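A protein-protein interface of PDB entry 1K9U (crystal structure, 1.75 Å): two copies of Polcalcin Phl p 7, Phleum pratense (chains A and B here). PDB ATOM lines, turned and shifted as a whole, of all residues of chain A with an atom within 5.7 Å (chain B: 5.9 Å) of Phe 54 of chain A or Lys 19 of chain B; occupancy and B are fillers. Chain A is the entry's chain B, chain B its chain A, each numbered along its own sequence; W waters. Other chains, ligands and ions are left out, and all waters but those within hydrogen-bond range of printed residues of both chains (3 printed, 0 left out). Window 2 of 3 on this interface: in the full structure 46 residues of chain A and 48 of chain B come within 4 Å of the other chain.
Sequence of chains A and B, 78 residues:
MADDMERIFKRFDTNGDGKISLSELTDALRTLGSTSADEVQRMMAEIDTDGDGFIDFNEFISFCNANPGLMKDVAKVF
N of Ile 20 of chain B lies within hydrogen-bond range of O of Ile 55 of chain A (2.8 Å).
OD1 of Asp 56 of chain A sits at hydrogen-bond distance from N of Glu 59 of chain A (2.8 Å). N of Glu 24 of chain B lies close to OG of Ser 21 of chain B (3.2 Å). The side-chain carboxylate (OD2) of Asp 13 of chain B sits at hydrogen-bond distance from the backbone NH (N) of Gly 18 of chain B, at 2.8 Å.
Among the printed residues, pairs that only touch across the chains: Met 44 of chain A with Ile 20 of chain B, Met 44 of chain A with Ser 21 of chain B, Met 44 of chain A with Leu 22 of chain B, Phe 54 of chain A with Lys 19 of chain B, Phe 54 of chain A with Ile 20 of chain B, Phe 54 of chain A with Ser 21 of chain B, Ile 55 of chain A with Phe 9 of chain B, Ile 55 of chain A with Lys 19 of chain B, Asp 56 of chain A with Phe 9 of chain B, Asp 56 of chain A with Gly 18 of chain B and Phe 57 of chain A with Phe 9 of chain B.
Gly 51 of chain A touches none of the printed residues of chain B. Asp 52 of chain A touches none of the printed residues of chain B. Of the printed residues of chain B, Ile 55 of chain A touches Phe 9, Lys 19 and Ile 20. Of the printed residues of chain B, Asp 56 of chain A touches Phe 9 and Gly 18. Of chain A, only Phe 54 and Ile 55 come within 4 Å of Lys 19 of chain B. Printed residues of chain A within 4 Å of Ile 20 of chain B: Met 44, Phe 54 and Ile 55. The nearest printed residue of chain B that does not touch Ile 55 of chain A is Gly 18 of chain B (4.5 Å).
Printed residues of chain B that touch a printed residue of chain A: Phe 9, Gly 18, Lys 19, Ile 20, Ser 21 and Leu 22. Hydrophobic or aromatic side chains of chain B that line the printed part of chain A: Phe 9 and Ile 20. Among the printed residues, 12 pairs touch across the chains.
No position is printed for both chains. Of the 12 pairs that touch across the chains among the printed residues, none has its exchanged pair printed and touching as well.
Water W3 bridges the backbone carbonyl oxygen (O) of Gly 18 of chain B (2.6 Å) and the backbone NH (N) of Phe 57 of chain A (3.0 Å). Water W2 bridges the side-chain amino group of Lys 19 of chain B and the side-chain carboxylate of Asp 52 of chain A. Water W1 lies within hydrogen-bond range of the backbone carbonyl oxygen of Gly 53 of chain A (3.0 Å) and the backbone NH of Leu 22 of chain B (3.0 Å).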
ATOM      1  N   MET A  44       0.372  -3.633   7.421  1.00  0.00           N
ATOM      2  CA  MET A  44       0.557  -2.979   8.712  1.00  0.00           C
ATOM      3  C   MET A  44       0.510  -1.458   8.540  1.00  0.00           C
ATOM      4  O   MET A  44      -0.141  -0.762   9.308  1.00  0.00           O
ATOM      5  CB  MET A  44       1.900  -3.391   9.329  1.00  0.00           C
ATOM      6  CG  MET A  44       2.253  -2.684  10.628  1.00  0.00           C
ATOM      7  SD  MET A  44       1.099  -3.020  11.968  1.00  0.00           S
ATOM      8  CE  MET A  44       1.667  -4.639  12.495  1.00  0.00           C
ATOM      9  N   ASP A  48      -1.807   0.885  10.862  1.00  0.00           N
ATOM     10  CA  ASP A  48      -1.025   1.527  11.922  1.00  0.00           C
ATOM     11  C   ASP A  48      -1.014   3.049  11.732  1.00  0.00           C
ATOM     12  O   ASP A  48      -0.032   3.626  11.258  1.00  0.00           O
ATOM     13  CB  ASP A  48       0.399   0.960  11.898  1.00  0.00           C
ATOM     14  CG  ASP A  48       1.341   1.671  12.846  1.00  0.00           C
ATOM     15  OD1 ASP A  48       0.899   2.129  13.923  1.00  0.00           O
ATOM     16  OD2 ASP A  48       2.543   1.747  12.512  1.00  0.00           O
ATOM     17  N   ASP A  50      -0.925   5.530  14.016  1.00  0.00           N
ATOM     18  CA  ASP A  50      -0.032   6.335  14.852  1.00  0.00           C
ATOM     19  C   ASP A  50       1.439   6.033  14.584  1.00  0.00           C
ATOM     20  O   ASP A  50       2.332   6.585  15.230  1.00  0.00           O
ATOM     21  CB  ASP A  50      -0.358   6.190  16.352  1.00  0.00           C
ATOM     22  CG  ASP A  50      -0.167   4.778  16.882  1.00  0.00           C
ATOM     23  OD1 ASP A  50       0.625   3.998  16.310  1.00  0.00           O
ATOM     24  OD2 ASP A  50      -0.810   4.462  17.909  1.00  0.00           O
ATOM     25  N   GLY A  51       1.678   5.154  13.614  1.00  0.00           N
ATOM     26  CA  GLY A  51       3.029   4.809  13.205  1.00  0.00           C
ATOM     27  C   GLY A  51       4.019   4.170  14.165  1.00  0.00           C
ATOM     28  O   GLY A  51       5.228   4.286  13.941  1.00  0.00           O
ATOM     29  N   ASP A  52       3.555   3.482  15.205  1.00  0.00           N
ATOM     30  CA  ASP A  52       4.501   2.861  16.129  1.00  0.00           C
ATOM     31  C   ASP A  52       4.910   1.444  15.727  1.00  0.00           C
ATOM     32  O   ASP A  52       5.691   0.799  16.426  1.00  0.00           O
ATOM     33  CB  ASP A  52       3.964   2.881  17.573  1.00  0.00           C
ATOM     34  CG  ASP A  52       2.724   2.030  17.759  1.00  0.00           C
ATOM     35  OD1 ASP A  52       2.252   1.443  16.770  1.00  0.00           O
ATOM     36  OD2 ASP A  52       2.223   1.955  18.906  1.00  0.00           O
ATOM     37  N   GLY A  53       4.395   0.967  14.596  1.00  0.00           N
ATOM     38  CA  GLY A  53       4.756  -0.362  14.127  1.00  0.00           C
ATOM     39  C   GLY A  53       3.883  -1.500  14.625  1.00  0.00           C
ATOM     40  O   GLY A  53       4.143  -2.667  14.318  1.00  0.00           O
ATOM     41  N   PHE A  54       2.857  -1.167  15.400  1.00  0.00           N
ATOM     42  CA  PHE A  54       1.939  -2.167  15.932  1.00  0.00           C
ATOM     43  C   PHE A  54       0.508  -1.704  15.713  1.00  0.00           C
ATOM     44  O   PHE A  54       0.259  -0.531  15.431  1.00  0.00           O
ATOM     45  CB  PHE A  54       2.135  -2.364  17.445  1.00  0.00           C
ATOM     46  CG  PHE A  54       3.524  -2.764  17.844  1.00  0.00           C
ATOM     47  CD1 PHE A  54       4.545  -1.818  17.912  1.00  0.00           C
ATOM     48  CD2 PHE A  54       3.813  -4.087  18.160  1.00  0.00           C
ATOM     49  CE1 PHE A  54       5.834  -2.189  18.293  1.00  0.00           C
ATOM     50  CE2 PHE A  54       5.098  -4.469  18.541  1.00  0.00           C
ATOM     51  CZ  PHE A  54       6.112  -3.517  18.608  1.00  0.00           C
ATOM     52  N   ILE A  55      -0.434  -2.628  15.848  1.00  0.00           N
ATOM     53  CA  ILE A  55      -1.840  -2.274  15.724  1.00  0.00           C
ATOM     54  C   ILE A  55      -2.428  -2.302  17.134  1.00  0.00           C
ATOM     55  O   ILE A  55      -2.527  -3.375  17.733  1.00  0.00           O
ATOM     56  CB  ILE A  55      -2.621  -3.297  14.873  1.00  0.00           C
ATOM     57  CG1 ILE A  55      -1.986  -3.421  13.488  1.00  0.00           C
ATOM     58  CG2 ILE A  55      -4.084  -2.868  14.759  1.00  0.00           C
ATOM     59  CD1 ILE A  55      -2.508  -4.596  12.674  1.00  0.00           C
ATOM     60  N   ASP A  56      -2.788  -1.149  17.696  1.00  0.00           N
ATOM     61  CA  ASP A  56      -3.390  -1.202  19.024  1.00  0.00           C
ATOM     62  C   ASP A  56      -4.905  -1.325  18.877  1.00  0.00           C
ATOM     63  O   ASP A  56      -5.430  -1.307  17.761  1.00  0.00           O
ATOM     64  CB  ASP A  56      -3.005   0.004  19.910  1.00  0.00           C
ATOM     65  CG  ASP A  56      -3.406   1.348  19.328  1.00  0.00           C
ATOM     66  OD1 ASP A  56      -4.402   1.428  18.593  1.00  0.00           O
ATOM     67  OD2 ASP A  56      -2.720   2.342  19.648  1.00  0.00           O
ATOM     68  N   PHE A  57      -5.609  -1.464  19.993  1.00  0.00           N
ATOM     69  CA  PHE A  57      -7.051  -1.643  19.932  1.00  0.00           C
ATOM     70  C   PHE A  57      -7.780  -0.454  19.313  1.00  0.00           C
ATOM     71  O   PHE A  57      -8.754  -0.643  18.590  1.00  0.00           O
ATOM     72  CB  PHE A  57      -7.602  -1.967  21.325  1.00  0.00           C
ATOM     73  CG  PHE A  57      -8.965  -2.613  21.307  1.00  0.00           C
ATOM     74  CD1 PHE A  57      -9.243  -3.669  20.436  1.00  0.00           C
ATOM     75  CD2 PHE A  57      -9.958  -2.191  22.183  1.00  0.00           C
ATOM     76  CE1 PHE A  57     -10.494  -4.293  20.440  1.00  0.00           C
ATOM     77  CE2 PHE A  57     -11.209  -2.807  22.199  1.00  0.00           C
ATOM     78  CZ  PHE A  57     -11.479  -3.859  21.328  1.00  0.00           C
ATOM     79  N   GLU A  59      -6.721   1.500  16.955  1.00  0.00           N
ATOM     80  CA  GLU A  59      -6.530   1.385  15.516  1.00  0.00           C
ATOM     81  C   GLU A  59      -7.353   0.244  14.936  1.00  0.00           C
ATOM     82  O   GLU A  59      -7.889   0.367  13.836  1.00  0.00           O
ATOM     83  CB  GLU A  59      -5.043   1.204  15.203  1.00  0.00           C
ATOM     84  CG  GLU A  59      -4.211   2.429  15.614  1.00  0.00           C
ATOM     85  CD  GLU A  59      -2.719   2.184  15.574  1.00  0.00           C
ATOM     86  OE1 GLU A  59      -2.293   1.047  15.846  1.00  0.00           O
ATOM     87  OE2 GLU A  59      -1.965   3.136  15.290  1.00  0.00           O
ATOM     88  N   PHE B   9      -9.281  -9.610  18.355  1.00  0.00           N
ATOM     89  CA  PHE B   9      -8.058  -8.874  18.672  1.00  0.00           C
ATOM     90  C   PHE B   9      -7.212  -9.681  19.654  1.00  0.00           C
ATOM     91  O   PHE B   9      -6.007  -9.856  19.466  1.00  0.00           O
ATOM     92  CB  PHE B   9      -8.404  -7.516  19.290  1.00  0.00           C
ATOM     93  CG  PHE B   9      -7.211  -6.625  19.499  1.00  0.00           C
ATOM     94  CD1 PHE B   9      -6.700  -5.863  18.449  1.00  0.00           C
ATOM     95  CD2 PHE B   9      -6.587  -6.560  20.741  1.00  0.00           C
ATOM     96  CE1 PHE B   9      -5.582  -5.049  18.633  1.00  0.00           C
ATOM     97  CE2 PHE B   9      -5.465  -5.750  20.939  1.00  0.00           C
ATOM     98  CZ  PHE B   9      -4.961  -4.993  19.881  1.00  0.00           C
ATOM     99  N   ASP B  13      -3.341 -11.295  19.494  1.00  0.00           N
ATOM    100  CA  ASP B  13      -2.347 -10.587  20.295  1.00  0.00           C
ATOM    101  C   ASP B  13      -1.704 -11.682  21.147  1.00  0.00           C
ATOM    102  O   ASP B  13      -1.997 -11.833  22.339  1.00  0.00           O
ATOM    103  CB  ASP B  13      -3.006  -9.531  21.186  1.00  0.00           C
ATOM    104  CG  ASP B  13      -2.026  -8.891  22.152  1.00  0.00           C
ATOM    105  OD1 ASP B  13      -0.803  -8.985  21.906  1.00  0.00           O
ATOM    106  OD2 ASP B  13      -2.479  -8.286  23.152  1.00  0.00           O
ATOM    107  N   ASN B  15       1.265 -12.286  22.658  1.00  0.00           N
ATOM    108  CA  ASN B  15       1.924 -12.028  23.935  1.00  0.00           C
ATOM    109  C   ASN B  15       1.123 -11.169  24.905  1.00  0.00           C
ATOM    110  O   ASN B  15       1.630 -10.766  25.950  1.00  0.00           O
ATOM    111  CB  ASN B  15       3.302 -11.407  23.695  1.00  0.00           C
ATOM    112  CG  ASN B  15       3.228 -10.008  23.115  1.00  0.00           C
ATOM    113  OD1 ASN B  15       2.171  -9.547  22.685  1.00  0.00           O
ATOM    114  ND2 ASN B  15       4.365  -9.324  23.097  1.00  0.00           N
ATOM    115  N   GLY B  16      -0.129 -10.901  24.552  1.00  0.00           N
ATOM    116  CA  GLY B  16      -1.015 -10.118  25.399  1.00  0.00           C
ATOM    117  C   GLY B  16      -0.565  -8.745  25.857  1.00  0.00           C
ATOM    118  O   GLY B  16      -0.950  -8.303  26.944  1.00  0.00           O
ATOM    119  N   ASP B  17       0.231  -8.050  25.054  1.00  0.00           N
ATOM    120  CA  ASP B  17       0.678  -6.722  25.455  1.00  0.00           C
ATOM    121  C   ASP B  17      -0.276  -5.626  24.984  1.00  0.00           C
ATOM    122  O   ASP B  17       0.010  -4.439  25.128  1.00  0.00           O
ATOM    123  CB  ASP B  17       2.105  -6.451  24.958  1.00  0.00           C
ATOM    124  CG  ASP B  17       2.220  -6.472  23.442  1.00  0.00           C
ATOM    125  OD1 ASP B  17       1.216  -6.772  22.764  1.00  0.00           O
ATOM    126  OD2 ASP B  17       3.326  -6.186  22.939  1.00  0.00           O
ATOM    127  N   GLY B  18      -1.414  -6.029  24.425  1.00  0.00           N
ATOM    128  CA  GLY B  18      -2.402  -5.062  23.977  1.00  0.00           C
ATOM    129  C   GLY B  18      -2.229  -4.517  22.574  1.00  0.00           C
ATOM    130  O   GLY B  18      -2.995  -3.653  22.150  1.00  0.00           O
ATOM    131  N   LYS B  19      -1.233  -5.007  21.842  1.00  0.00           N
ATOM    132  CA  LYS B  19      -1.020  -4.532  20.479  1.00  0.00           C
ATOM    133  C   LYS B  19      -0.588  -5.667  19.565  1.00  0.00           C
ATOM    134  O   LYS B  19       0.069  -6.614  20.000  1.00  0.00           O
ATOM    135  CB  LYS B  19       0.015  -3.402  20.457  1.00  0.00           C
ATOM    136  CG  LYS B  19       1.390  -3.783  20.967  1.00  0.00           C
ATOM    137  CD  LYS B  19       2.238  -2.544  21.231  1.00  0.00           C
ATOM    138  CE  LYS B  19       3.637  -2.933  21.689  1.00  0.00           C
ATOM    139  NZ  LYS B  19       4.488  -1.751  21.990  1.00  0.00           N
ATOM    140  N   ILE B  20      -0.968  -5.571  18.294  1.00  0.00           N
ATOM    141  CA  ILE B  20      -0.624  -6.599  17.317  1.00  0.00           C
ATOM    142  C   ILE B  20       0.664  -6.242  16.582  1.00  0.00           C
ATOM    143  O   ILE B  20       0.734  -5.225  15.894  1.00  0.00           O
ATOM    144  CB  ILE B  20      -1.749  -6.778  16.272  1.00  0.00           C
ATOM    145  CG1 ILE B  20      -3.087  -7.025  16.977  1.00  0.00           C
ATOM    146  CG2 ILE B  20      -1.403  -7.935  15.332  1.00  0.00           C
ATOM    147  CD1 ILE B  20      -3.118  -8.258  17.867  1.00  0.00           C
ATOM    148  N   SER B  21       1.680  -7.090  16.735  1.00  0.00           N
ATOM    149  CA  SER B  21       2.970  -6.875  16.086  1.00  0.00           C
ATOM    150  C   SER B  21       2.985  -7.411  14.657  1.00  0.00           C
ATOM    151  O   SER B  21       2.020  -8.005  14.192  1.00  0.00           O
ATOM    152  CB  SER B  21       4.073  -7.576  16.885  1.00  0.00           C
ATOM    153  OG  SER B  21       3.921  -8.982  16.796  1.00  0.00           O
ATOM    154  N   LEU B  22       4.098  -7.208  13.964  1.00  0.00           N
ATOM    155  CA  LEU B  22       4.215  -7.688  12.595  1.00  0.00           C
ATOM    156  C   LEU B  22       4.113  -9.211  12.560  1.00  0.00           C
ATOM    157  O   LEU B  22       3.444  -9.774  11.696  1.00  0.00           O
ATOM    158  CB  LEU B  22       5.551  -7.252  11.996  1.00  0.00           C
ATOM    159  CG  LEU B  22       5.716  -7.424  10.487  1.00  0.00           C
ATOM    160  CD1 LEU B  22       4.683  -6.573   9.749  1.00  0.00           C
ATOM    161  CD2 LEU B  22       7.129  -7.006  10.104  1.00  0.00           C
ATOM    162  N   GLU B  24       2.656 -11.125  14.768  1.00  0.00           N
ATOM    163  CA  GLU B  24       1.313 -11.526  15.155  1.00  0.00           C
ATOM    164  C   GLU B  24       0.337 -11.310  14.006  1.00  0.00           C
ATOM    165  O   GLU B  24      -0.595 -12.088  13.829  1.00  0.00           O
ATOM    166  CB  GLU B  24       0.872 -10.758  16.406  1.00  0.00           C
ATOM    167  CG  GLU B  24       1.702 -11.130  17.637  1.00  0.00           C
ATOM    168  CD  GLU B  24       1.412 -10.270  18.851  1.00  0.00           C
ATOM    169  OE1 GLU B  24       0.875  -9.157  18.684  1.00  0.00           O
ATOM    170  OE2 GLU B  24       1.743 -10.699  19.979  1.00  0.00           O
HETATM  171  O   HOH W   1       5.799  -5.007  15.023  1.00  0.00           O
HETATM  172  O   HOH W   2       4.148   0.741  20.895  1.00  0.00           O
HETATM  173  O   HOH W   3      -4.431  -1.562  22.747  1.00  0.00           O
